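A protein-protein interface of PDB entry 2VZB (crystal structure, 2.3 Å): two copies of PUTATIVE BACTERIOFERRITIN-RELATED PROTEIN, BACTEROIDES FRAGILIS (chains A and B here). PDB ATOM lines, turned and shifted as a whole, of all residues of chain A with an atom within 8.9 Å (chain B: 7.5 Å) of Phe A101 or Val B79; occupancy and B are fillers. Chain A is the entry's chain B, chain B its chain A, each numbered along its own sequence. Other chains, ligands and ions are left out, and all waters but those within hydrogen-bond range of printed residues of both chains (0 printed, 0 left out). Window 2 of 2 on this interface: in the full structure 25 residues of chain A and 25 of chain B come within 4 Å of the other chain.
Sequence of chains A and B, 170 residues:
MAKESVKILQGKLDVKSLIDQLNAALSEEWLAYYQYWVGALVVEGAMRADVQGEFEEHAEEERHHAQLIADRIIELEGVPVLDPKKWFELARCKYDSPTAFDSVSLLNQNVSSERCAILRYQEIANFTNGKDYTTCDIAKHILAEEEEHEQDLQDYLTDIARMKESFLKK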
ATOM      1  N   TYR A  34       0.105   2.757 -29.768  1.00  0.00           N
ATOM      2  CA  TYR A  34       1.258   2.615 -28.872  1.00  0.00           C
ATOM      3  C   TYR A  34       2.531   3.239 -29.442  1.00  0.00           C
ATOM      4  O   TYR A  34       3.322   3.866 -28.730  1.00  0.00           O
ATOM      5  CB  TYR A  34       1.540   1.149 -28.559  1.00  0.00           C
ATOM      6  CG  TYR A  34       2.437   1.012 -27.361  1.00  0.00           C
ATOM      7  CD1 TYR A  34       1.927   1.174 -26.078  1.00  0.00           C
ATOM      8  CD2 TYR A  34       3.802   0.765 -27.501  1.00  0.00           C
ATOM      9  CE1 TYR A  34       2.740   1.059 -24.950  1.00  0.00           C
ATOM     10  CE2 TYR A  34       4.632   0.636 -26.372  1.00  0.00           C
ATOM     11  CZ  TYR A  34       4.081   0.781 -25.102  1.00  0.00           C
ATOM     12  OH  TYR A  34       4.858   0.674 -23.977  1.00  0.00           O
ATOM     13  N   VAL A  38       4.499   5.980 -27.240  1.00  0.00           N
ATOM     14  CA  VAL A  38       5.845   5.787 -26.712  1.00  0.00           C
ATOM     15  C   VAL A  38       6.807   6.708 -27.429  1.00  0.00           C
ATOM     16  O   VAL A  38       7.716   7.243 -26.817  1.00  0.00           O
ATOM     17  CB  VAL A  38       6.291   4.288 -26.752  1.00  0.00           C
ATOM     18  CG1 VAL A  38       6.657   3.828 -28.155  1.00  0.00           C
ATOM     19  CG2 VAL A  38       7.464   4.071 -25.758  1.00  0.00           C
ATOM     20  N   GLY A  39       6.577   6.915 -28.727  1.00  0.00           N
ATOM     21  CA  GLY A  39       7.343   7.905 -29.509  1.00  0.00           C
ATOM     22  C   GLY A  39       7.303   9.296 -28.890  1.00  0.00           C
ATOM     23  O   GLY A  39       8.330   9.983 -28.787  1.00  0.00           O
ATOM     24  N   ALA A  40       6.110   9.702 -28.463  1.00  0.00           N
ATOM     25  CA  ALA A  40       5.918  10.967 -27.767  1.00  0.00           C
ATOM     26  C   ALA A  40       6.770  10.997 -26.498  1.00  0.00           C
ATOM     27  O   ALA A  40       7.377  12.006 -26.170  1.00  0.00           O
ATOM     28  CB  ALA A  40       4.420  11.180 -27.418  1.00  0.00           C
ATOM     29  N   LEU A  41       6.817   9.887 -25.794  1.00  0.00           N
ATOM     30  CA  LEU A  41       7.586   9.803 -24.542  1.00  0.00           C
ATOM     31  C   LEU A  41       9.117   9.934 -24.699  1.00  0.00           C
ATOM     32  O   LEU A  41       9.798  10.337 -23.782  1.00  0.00           O
ATOM     33  CB  LEU A  41       7.251   8.490 -23.811  1.00  0.00           C
ATOM     34  CG  LEU A  41       5.899   8.465 -23.088  1.00  0.00           C
ATOM     35  CD1 LEU A  41       5.429   7.017 -22.817  1.00  0.00           C
ATOM     36  CD2 LEU A  41       5.995   9.319 -21.777  1.00  0.00           C
ATOM     37  N   VAL A  42       9.644   9.583 -25.862  1.00  0.00           N
ATOM     38  CA  VAL A  42      11.099   9.539 -26.078  1.00  0.00           C
ATOM     39  C   VAL A  42      11.656  10.518 -27.129  1.00  0.00           C
ATOM     40  O   VAL A  42      12.870  10.682 -27.225  1.00  0.00           O
ATOM     41  CB  VAL A  42      11.569   8.108 -26.439  1.00  0.00           C
ATOM     42  CG1 VAL A  42      11.134   7.135 -25.359  1.00  0.00           C
ATOM     43  CG2 VAL A  42      11.071   7.697 -27.835  1.00  0.00           C
ATOM     44  N   VAL A  43      10.792  11.145 -27.924  1.00  0.00           N
ATOM     45  CA  VAL A  43      11.268  12.044 -28.981  1.00  0.00           C
ATOM     46  C   VAL A  43      12.170  13.168 -28.435  1.00  0.00           C
ATOM     47  O   VAL A  43      11.932  13.723 -27.380  1.00  0.00           O
ATOM     48  CB  VAL A  43      10.119  12.650 -29.847  1.00  0.00           C
ATOM     49  CG1 VAL A  43       9.163  13.534 -29.020  1.00  0.00           C
ATOM     50  CG2 VAL A  43      10.700  13.403 -31.033  1.00  0.00           C
ATOM     51  N   GLU A  44      13.220  13.468 -29.190  1.00  0.00           N
ATOM     52  CA  GLU A  44      14.186  14.527 -28.870  1.00  0.00           C
ATOM     53  C   GLU A  44      14.620  15.222 -30.148  1.00  0.00           C
ATOM     54  O   GLU A  44      14.606  14.628 -31.234  1.00  0.00           O
ATOM     55  CB  GLU A  44      15.457  13.962 -28.271  1.00  0.00           C
ATOM     56  CG  GLU A  44      15.310  13.174 -27.013  1.00  0.00           C
ATOM     57  CD  GLU A  44      16.663  12.666 -26.544  1.00  0.00           C
ATOM     58  OE1 GLU A  44      17.660  12.899 -27.266  1.00  0.00           O
ATOM     59  OE2 GLU A  44      16.734  12.054 -25.456  1.00  0.00           O
ATOM     60  N   GLY A  45      15.029  16.472 -29.992  1.00  0.00           N
ATOM     61  CA  GLY A  45      15.678  17.220 -31.062  1.00  0.00           C
ATOM     62  C   GLY A  45      14.866  18.338 -31.667  1.00  0.00           C
ATOM     63  O   GLY A  45      14.099  19.025 -30.984  1.00  0.00           O
ATOM     64  N   ALA A  46      15.053  18.499 -32.976  1.00  0.00           N
ATOM     65  CA  ALA A  46      14.434  19.572 -33.746  1.00  0.00           C
ATOM     66  C   ALA A  46      12.915  19.544 -33.608  1.00  0.00           C
ATOM     67  O   ALA A  46      12.292  18.497 -33.773  1.00  0.00           O
ATOM     68  CB  ALA A  46      14.834  19.486 -35.216  1.00  0.00           C
ATOM     69  N   ARG A  48      10.973  19.472 -31.171  1.00  0.00           N
ATOM     70  CA  ARG A  48      10.509  18.370 -30.305  1.00  0.00           C
ATOM     71  C   ARG A  48       9.117  18.629 -29.707  1.00  0.00           C
ATOM     72  O   ARG A  48       8.253  17.766 -29.780  1.00  0.00           O
ATOM     73  CB  ARG A  48      11.506  18.060 -29.187  1.00  0.00           C
ATOM     74  CG  ARG A  48      11.175  16.781 -28.351  1.00  0.00           C
ATOM     75  CD  ARG A  48      10.311  17.068 -27.112  1.00  0.00           C
ATOM     76  NE  ARG A  48      10.869  18.177 -26.351  1.00  0.00           N
ATOM     77  CZ  ARG A  48      10.214  18.937 -25.482  1.00  0.00           C
ATOM     78  NH1 ARG A  48       8.940  18.706 -25.207  1.00  0.00           N
ATOM     79  NH2 ARG A  48      10.855  19.942 -24.885  1.00  0.00           N
ATOM     80  N   VAL A  51       6.447  18.180 -32.305  1.00  0.00           N
ATOM     81  CA  VAL A  51       6.401  16.801 -32.796  1.00  0.00           C
ATOM     82  C   VAL A  51       5.852  15.887 -31.698  1.00  0.00           C
ATOM     83  O   VAL A  51       5.042  15.002 -31.955  1.00  0.00           O
ATOM     84  CB  VAL A  51       7.805  16.276 -33.274  1.00  0.00           C
ATOM     85  CG1 VAL A  51       7.770  14.767 -33.567  1.00  0.00           C
ATOM     86  CG2 VAL A  51       8.310  17.066 -34.508  1.00  0.00           C
ATOM     87  N   PHE A  55       2.388  13.623 -31.878  1.00  0.00           N
ATOM     88  CA  PHE A  55       2.398  12.205 -31.529  1.00  0.00           C
ATOM     89  C   PHE A  55       1.348  11.915 -30.471  1.00  0.00           C
ATOM     90  O   PHE A  55       0.619  10.927 -30.567  1.00  0.00           O
ATOM     91  CB  PHE A  55       3.769  11.761 -31.018  1.00  0.00           C
ATOM     92  CG  PHE A  55       4.843  11.669 -32.087  1.00  0.00           C
ATOM     93  CD1 PHE A  55       4.562  11.854 -33.441  1.00  0.00           C
ATOM     94  CD2 PHE A  55       6.142  11.340 -31.722  1.00  0.00           C
ATOM     95  CE1 PHE A  55       5.569  11.740 -34.396  1.00  0.00           C
ATOM     96  CE2 PHE A  55       7.141  11.228 -32.669  1.00  0.00           C
ATOM     97  CZ  PHE A  55       6.863  11.431 -34.007  1.00  0.00           C
ATOM     98  N   SER A  97       9.363  -0.200 -33.937  1.00  0.00           N
ATOM     99  CA  SER A  97       9.873   0.188 -32.619  1.00  0.00           C
ATOM    100  C   SER A  97      10.866   1.366 -32.689  1.00  0.00           C
ATOM    101  O   SER A  97      11.709   1.445 -33.604  1.00  0.00           O
ATOM    102  CB  SER A  97      10.541  -1.016 -31.947  1.00  0.00           C
ATOM    103  OG  SER A  97      10.817  -0.773 -30.578  1.00  0.00           O
ATOM    104  N   PRO A  98      10.752   2.313 -31.742  1.00  0.00           N
ATOM    105  CA  PRO A  98      11.786   3.338 -31.645  1.00  0.00           C
ATOM    106  C   PRO A  98      13.166   2.762 -31.323  1.00  0.00           C
ATOM    107  O   PRO A  98      13.323   1.991 -30.370  1.00  0.00           O
ATOM    108  CB  PRO A  98      11.306   4.222 -30.484  1.00  0.00           C
ATOM    109  CG  PRO A  98       9.864   3.941 -30.341  1.00  0.00           C
ATOM    110  CD  PRO A  98       9.666   2.530 -30.768  1.00  0.00           C
ATOM    111  N   THR A  99      14.144   3.152 -32.129  1.00  0.00           N
ATOM    112  CA  THR A  99      15.545   2.853 -31.865  1.00  0.00           C
ATOM    113  C   THR A  99      16.250   4.207 -31.686  1.00  0.00           C
ATOM    114  O   THR A  99      16.615   4.589 -30.584  1.00  0.00           O
ATOM    115  CB  THR A  99      16.162   2.008 -33.005  1.00  0.00           C
ATOM    116  OG1 THR A  99      16.042   2.702 -34.249  1.00  0.00           O
ATOM    117  CG2 THR A  99      15.445   0.659 -33.113  1.00  0.00           C
ATOM    118  N   ALA A 100      16.384   4.947 -32.776  1.00  0.00           N
ATOM    119  CA  ALA A 100      16.834   6.339 -32.716  1.00  0.00           C
ATOM    120  C   ALA A 100      15.670   7.231 -32.206  1.00  0.00           C
ATOM    121  O   ALA A 100      14.541   7.111 -32.668  1.00  0.00           O
ATOM    122  CB  ALA A 100      17.318   6.801 -34.080  1.00  0.00           C
ATOM    123  N   PHE A 101      15.974   8.094 -31.241  1.00  0.00           N
ATOM    124  CA  PHE A 101      14.972   8.944 -30.571  1.00  0.00           C
ATOM    125  C   PHE A 101      14.821  10.347 -31.166  1.00  0.00           C
ATOM    126  O   PHE A 101      13.960  11.109 -30.750  1.00  0.00           O
ATOM    127  CB  PHE A 101      15.283   9.073 -29.075  1.00  0.00           C
ATOM    128  CG  PHE A 101      15.090   7.804 -28.292  1.00  0.00           C
ATOM    129  CD1 PHE A 101      14.483   6.676 -28.867  1.00  0.00           C
ATOM    130  CD2 PHE A 101      15.462   7.756 -26.954  1.00  0.00           C
ATOM    131  CE1 PHE A 101      14.294   5.515 -28.135  1.00  0.00           C
ATOM    132  CE2 PHE A 101      15.272   6.598 -26.207  1.00  0.00           C
ATOM    133  CZ  PHE A 101      14.689   5.468 -26.802  1.00  0.00           C
ATOM    134  N   ASP A 102      15.647  10.668 -32.150  1.00  0.00           N
ATOM    135  CA  ASP A 102      15.590  11.974 -32.805  1.00  0.00           C
ATOM    136  C   ASP A 102      14.319  12.081 -33.632  1.00  0.00           C
ATOM    137  O   ASP A 102      13.776  11.074 -34.128  1.00  0.00           O
ATOM    138  CB  ASP A 102      16.809  12.232 -33.698  1.00  0.00           C
ATOM    139  CG  ASP A 102      16.811  11.370 -34.902  1.00  0.00           C
ATOM    140  OD1 ASP A 102      16.610  11.893 -36.013  1.00  0.00           O
ATOM    141  OD2 ASP A 102      16.953  10.143 -34.718  1.00  0.00           O
ATOM    142  N   SER A 103      13.865  13.313 -33.796  1.00  0.00           N
ATOM    143  CA  SER A 103      12.530  13.542 -34.324  1.00  0.00           C
ATOM    144  C   SER A 103      12.382  13.096 -35.788  1.00  0.00           C
ATOM    145  O   SER A 103      11.358  12.512 -36.147  1.00  0.00           O
ATOM    146  CB  SER A 103      12.080  14.995 -34.077  1.00  0.00           C
ATOM    147  OG  SER A 103      12.999  15.946 -34.554  1.00  0.00           O
ATOM    148  N   VAL A 104      13.418  13.316 -36.607  1.00  0.00           N
ATOM    149  CA  VAL A 104      13.390  12.856 -38.029  1.00  0.00           C
ATOM    150  C   VAL A 104      13.192  11.322 -38.112  1.00  0.00           C
ATOM    151  O   VAL A 104      12.382  10.818 -38.905  1.00  0.00           O
ATOM    152  CB  VAL A 104      14.655  13.277 -38.834  1.00  0.00           C
ATOM    153  CG1 VAL A 104      14.688  12.606 -40.226  1.00  0.00           C
ATOM    154  CG2 VAL A 104      14.722  14.799 -38.991  1.00  0.00           C
ATOM    155  N   SER A 105      13.920  10.593 -37.280  1.00  0.00           N
ATOM    156  CA  SER A 105      13.816   9.134 -37.264  1.00  0.00           C
ATOM    157  C   SER A 105      12.406   8.696 -36.914  1.00  0.00           C
ATOM    158  O   SER A 105      11.816   7.853 -37.596  1.00  0.00           O
ATOM    159  CB  SER A 105      14.799   8.503 -36.264  1.00  0.00           C
ATOM    160  OG  SER A 105      16.144   8.820 -36.591  1.00  0.00           O
ATOM    161  N   LEU A 106      11.879   9.270 -35.836  1.00  0.00           N
ATOM    162  CA  LEU A 106      10.519   8.936 -35.368  1.00  0.00           C
ATOM    163  C   LEU A 106       9.431   9.385 -36.357  1.00  0.00           C
ATOM    164  O   LEU A 106       8.476   8.659 -36.615  1.00  0.00           O
ATOM    165  CB  LEU A 106      10.282   9.491 -33.976  1.00  0.00           C
ATOM    166  CG  LEU A 106      11.161   8.831 -32.914  1.00  0.00           C
ATOM    167  CD1 LEU A 106      11.056   9.501 -31.530  1.00  0.00           C
ATOM    168  CD2 LEU A 106      10.832   7.339 -32.807  1.00  0.00           C
ATOM    169  N   LEU A 107       9.611  10.555 -36.936  1.00  0.00           N
ATOM    170  CA  LEU A 107       8.708  11.057 -37.970  1.00  0.00           C
ATOM    171  C   LEU A 107       8.635  10.103 -39.180  1.00  0.00           C
ATOM    172  O   LEU A 107       7.547   9.817 -39.715  1.00  0.00           O
ATOM    173  CB  LEU A 107       9.128  12.463 -38.435  1.00  0.00           C
ATOM    174  CG  LEU A 107       8.825  13.639 -37.494  1.00  0.00           C
ATOM    175  CD1 LEU A 107       9.690  14.866 -37.844  1.00  0.00           C
ATOM    176  CD2 LEU A 107       7.328  13.981 -37.523  1.00  0.00           C
ATOM    177  N   GLN A 109       9.415   6.852 -39.335  1.00  0.00           N
ATOM    178  CA  GLN A 109       8.757   5.615 -38.910  1.00  0.00           C
ATOM    179  C   GLN A 109       7.247   5.771 -38.919  1.00  0.00           C
ATOM    180  O   GLN A 109       6.534   4.936 -39.465  1.00  0.00           O
ATOM    181  CB  GLN A 109       9.220   5.201 -37.518  1.00  0.00           C
ATOM    182  CG  GLN A 109      10.656   4.684 -37.492  1.00  0.00           C
ATOM    183  CD  GLN A 109      11.077   4.186 -36.127  1.00  0.00           C
ATOM    184  OE1 GLN A 109      11.096   4.952 -35.169  1.00  0.00           O
ATOM    185  NE2 GLN A 109      11.438   2.896 -36.036  1.00  0.00           N
ATOM    186  N   ILE B  19      13.013   1.792 -11.701  1.00  0.00           N
ATOM    187  CA  ILE B  19      12.633   1.902 -13.122  1.00  0.00           C
ATOM    188  C   ILE B  19      12.129   0.562 -13.658  1.00  0.00           C
ATOM    189  O   ILE B  19      11.093   0.507 -14.320  1.00  0.00           O
ATOM    190  CB  ILE B  19      13.793   2.443 -13.992  1.00  0.00           C
ATOM    191  CG1 ILE B  19      14.061   3.921 -13.652  1.00  0.00           C
ATOM    192  CG2 ILE B  19      13.479   2.274 -15.470  1.00  0.00           C
ATOM    193  CD1 ILE B  19      15.331   4.490 -14.267  1.00  0.00           C
ATOM    194  N   ASN B  23       8.499  -0.214 -15.209  1.00  0.00           N
ATOM    195  CA  ASN B  23       8.279  -0.776 -16.555  1.00  0.00           C
ATOM    196  C   ASN B  23       7.480  -2.082 -16.562  1.00  0.00           C
ATOM    197  O   ASN B  23       6.796  -2.394 -17.526  1.00  0.00           O
ATOM    198  CB  ASN B  23       9.599  -0.956 -17.306  1.00  0.00           C
ATOM    199  CG  ASN B  23       9.925   0.240 -18.177  1.00  0.00           C
ATOM    200  OD1 ASN B  23       9.036   0.769 -18.855  1.00  0.00           O
ATOM    201  ND2 ASN B  23      11.194   0.676 -18.166  1.00  0.00           N
ATOM    202  N   LEU B  26       4.051  -0.656 -15.943  1.00  0.00           N
ATOM    203  CA  LEU B  26       3.586  -0.050 -17.199  1.00  0.00           C
ATOM    204  C   LEU B  26       3.027  -1.111 -18.148  1.00  0.00           C
ATOM    205  O   LEU B  26       1.916  -0.998 -18.685  1.00  0.00           O
ATOM    206  CB  LEU B  26       4.735   0.720 -17.874  1.00  0.00           C
ATOM    207  CG  LEU B  26       4.450   1.433 -19.190  1.00  0.00           C
ATOM    208  CD1 LEU B  26       3.213   2.327 -19.048  1.00  0.00           C
ATOM    209  CD2 LEU B  26       5.675   2.240 -19.639  1.00  0.00           C
ATOM    210  N   ALA B  70       4.631   6.077 -16.989  1.00  0.00           N
ATOM    211  CA  ALA B  70       5.577   6.373 -18.080  1.00  0.00           C
ATOM    212  C   ALA B  70       6.240   7.735 -17.915  1.00  0.00           C
ATOM    213  O   ALA B  70       7.455   7.869 -18.128  1.00  0.00           O
ATOM    214  CB  ALA B  70       4.895   6.287 -19.421  1.00  0.00           C
ATOM    215  N   ILE B  73       8.881   7.454 -15.203  1.00  0.00           N
ATOM    216  CA  ILE B  73      10.057   6.749 -15.743  1.00  0.00           C
ATOM    217  C   ILE B  73      10.993   7.748 -16.466  1.00  0.00           C
ATOM    218  O   ILE B  73      12.210   7.799 -16.228  1.00  0.00           O
ATOM    219  CB  ILE B  73       9.659   5.626 -16.708  1.00  0.00           C
ATOM    220  CG1 ILE B  73       9.031   4.457 -15.931  1.00  0.00           C
ATOM    221  CG2 ILE B  73      10.896   5.179 -17.537  1.00  0.00           C
ATOM    222  CD1 ILE B  73       8.391   3.387 -16.821  1.00  0.00           C
ATOM    223  N   ILE B  74      10.407   8.558 -17.337  1.00  0.00           N
ATOM    224  CA  ILE B  74      11.169   9.592 -18.038  1.00  0.00           C
ATOM    225  C   ILE B  74      11.858  10.544 -17.045  1.00  0.00           C
ATOM    226  O   ILE B  74      13.018  10.907 -17.220  1.00  0.00           O
ATOM    227  CB  ILE B  74      10.287  10.386 -19.006  1.00  0.00           C
ATOM    228  CG1 ILE B  74       9.765   9.482 -20.132  1.00  0.00           C
ATOM    229  CG2 ILE B  74      11.039  11.603 -19.598  1.00  0.00           C
ATOM    230  CD1 ILE B  74      10.832   8.860 -21.017  1.00  0.00           C
ATOM    231  N   LEU B  76      12.826   9.827 -14.075  1.00  0.00           N
ATOM    232  CA  LEU B  76      13.868   9.055 -13.411  1.00  0.00           C
ATOM    233  C   LEU B  76      15.000   8.682 -14.385  1.00  0.00           C
ATOM    234  O   LEU B  76      15.813   7.817 -14.098  1.00  0.00           O
ATOM    235  CB  LEU B  76      13.264   7.799 -12.783  1.00  0.00           C
ATOM    236  CG  LEU B  76      12.307   8.037 -11.604  1.00  0.00           C
ATOM    237  CD1 LEU B  76      11.517   6.754 -11.235  1.00  0.00           C
ATOM    238  CD2 LEU B  76      13.078   8.606 -10.402  1.00  0.00           C
ATOM    239  N   GLU B  77      15.037   9.352 -15.536  1.00  0.00           N
ATOM    240  CA  GLU B  77      16.035   9.107 -16.587  1.00  0.00           C
ATOM    241  C   GLU B  77      15.998   7.679 -17.154  1.00  0.00           C
ATOM    242  O   GLU B  77      17.011   7.169 -17.634  1.00  0.00           O
ATOM    243  CB  GLU B  77      17.452   9.454 -16.086  1.00  0.00           C
ATOM    244  CG  GLU B  77      17.622  10.928 -15.745  1.00  0.00           C
ATOM    245  CD  GLU B  77      17.510  11.833 -16.959  1.00  0.00           C
ATOM    246  OE1 GLU B  77      18.189  11.576 -17.967  1.00  0.00           O
ATOM    247  OE2 GLU B  77      16.737  12.813 -16.912  1.00  0.00           O
ATOM    248  N   GLY B  78      14.824   7.050 -17.094  1.00  0.00           N
ATOM    249  CA  GLY B  78      14.615   5.719 -17.648  1.00  0.00           C
ATOM    250  C   GLY B  78      13.985   5.802 -19.030  1.00  0.00           C
ATOM    251  O   GLY B  78      13.639   6.891 -19.513  1.00  0.00           O
ATOM    252  N   VAL B  79      13.856   4.641 -19.672  1.00  0.00           N
ATOM    253  CA  VAL B  79      13.164   4.525 -20.952  1.00  0.00           C
ATOM    254  C   VAL B  79      11.977   3.585 -20.765  1.00  0.00           C
ATOM    255  O   VAL B  79      12.150   2.455 -20.300  1.00  0.00           O
ATOM    256  CB  VAL B  79      14.097   3.982 -22.057  1.00  0.00           C
ATOM    257  CG1 VAL B  79      13.355   3.826 -23.410  1.00  0.00           C
ATOM    258  CG2 VAL B  79      15.306   4.888 -22.213  1.00  0.00           C
ATOM    259  N   PRO B  80      10.757   4.055 -21.090  1.00  0.00           N
ATOM    260  CA  PRO B  80       9.631   3.132 -20.965  1.00  0.00           C
ATOM    261  C   PRO B  80       9.699   2.054 -22.042  1.00  0.00           C
ATOM    262  O   PRO B  80      10.298   2.270 -23.095  1.00  0.00           O
ATOM    263  CB  PRO B  80       8.399   4.036 -21.165  1.00  0.00           C
ATOM    264  CG  PRO B  80       8.892   5.170 -21.991  1.00  0.00           C
ATOM    265  CD  PRO B  80      10.325   5.386 -21.563  1.00  0.00           C
ATOM    266  N   VAL B  81       9.064   0.920 -21.768  1.00  0.00           N
ATOM    267  CA  VAL B  81       9.034  -0.179 -22.711  1.00  0.00           C
ATOM    268  C   VAL B  81       8.556   0.317 -24.077  1.00  0.00           C
ATOM    269  O   VAL B  81       7.485   0.913 -24.209  1.00  0.00           O
ATOM    270  CB  VAL B  81       8.194  -1.406 -22.209  1.00  0.00           C
ATOM    271  CG1 VAL B  81       6.868  -0.974 -21.583  1.00  0.00           C
ATOM    272  CG2 VAL B  81       7.979  -2.389 -23.344  1.00  0.00           C
ATOM    273  N   LEU B  82       9.375   0.055 -25.085  1.00  0.00           N
ATOM    274  CA  LEU B  82       9.215   0.632 -26.415  1.00  0.00           C
ATOM    275  C   LEU B  82       8.446  -0.239 -27.383  1.00  0.00           C
ATOM    276  O   LEU B  82       8.153   0.183 -28.493  1.00  0.00           O
ATOM    277  CB  LEU B  82      10.587   0.881 -27.020  1.00  0.00           C
ATOM    278  CG  LEU B  82      11.547   1.781 -26.251  1.00  0.00           C
ATOM    279  CD1 LEU B  82      12.934   1.667 -26.888  1.00  0.00           C
ATOM    280  CD2 LEU B  82      11.072   3.209 -26.256  1.00  0.00           C
ATOM    281  N   LYS B  86       7.268  -6.860 -25.709  1.00  0.00           N
ATOM    282  CA  LYS B  86       7.923  -6.995 -24.402  1.00  0.00           C
ATOM    283  C   LYS B  86       6.995  -6.938 -23.185  1.00  0.00           C
ATOM    284  O   LYS B  86       7.421  -7.272 -22.087  1.00  0.00           O
ATOM    285  CB  LYS B  86       8.990  -5.910 -24.235  1.00  0.00           C
ATOM    286  CG  LYS B  86      10.266  -6.156 -25.034  1.00  0.00           C
ATOM    287  CD  LYS B  86      11.303  -5.034 -24.793  1.00  0.00           C
ATOM    288  CE  LYS B  86      11.896  -5.048 -23.336  1.00  0.00           C
ATOM    289  NZ  LYS B  86      12.089  -3.653 -22.781  1.00  0.00           N
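The backbone carbonyl oxygen (O) of Val B81 sits at hydrogen-bond distance from the side-chain hydroxyl (OH) of Tyr A34 (2.6 Å).
The side-chain amide nitrogen (ND2) of Asn B23 sits at hydrogen-bond distance from the backbone carbonyl oxygen (O) of Val B79 (2.9 Å).
The backbone NH of Val B81 sits at hydrogen-bond distance from the side-chain amide oxygen of Asn B23 (2.9 Å).
The backbone NH (N) of Glu A44 lies within hydrogen-bond range of the backbone carbonyl oxygen (O) of Phe A101.
The backbone carbonyl oxygen of Ser A97 lies within hydrogen-bond range of the side-chain amide nitrogen of Gln A109, 2.8 Å away.
Among the printed residues, merely in contact across the chains: Leu A41 with Ile B74 (3.3 Å), Leu A41 with Ala B70 (3.5 Å), Ser A97 with Leu B82 (3.5 Å), Val A38 with Val B81 (3.5 Å), Pro A98 with Leu B82 (3.5 Å), Val A38 with Leu B82 (3.7 Å) and Phe A101 with Val B79 (3.998 Å).
Printed residues of chain B within 4 Å of Phe A101: Val B79 (3.998 Å).
Of the printed residues of chain A, Val B79 touches Phe A101.
Of the printed residues of chain A, Ile B74 touches Leu A41 (3.3 Å).
Printed residues of chain B within 4 Å of Ser A97: Leu B82.
Printed residues of chain A within 4 Å of Leu B82: Val A38, Ser A97 and Pro A98.
Of the printed residues of chain B, Tyr A34 touches Val B81.
Of the printed residues of chain A, Ala B70 touches Leu A41.
Printed residues of chain B that touch a printed residue of chain A: Ala B70, Ile B74, Val B79, Val B81 and Leu B82.
Among the printed residues, 8 pairs touch across the chains.
Among the printed residues, no Asp or Glu carboxylate lies within 4 Å of a Lys or Arg side-chain nitrogen of the other chain.
No position is printed for both chains.
Of the 8 pairs that touch across the chains among the printed residues, none has its exchanged pair printed and touching as well.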
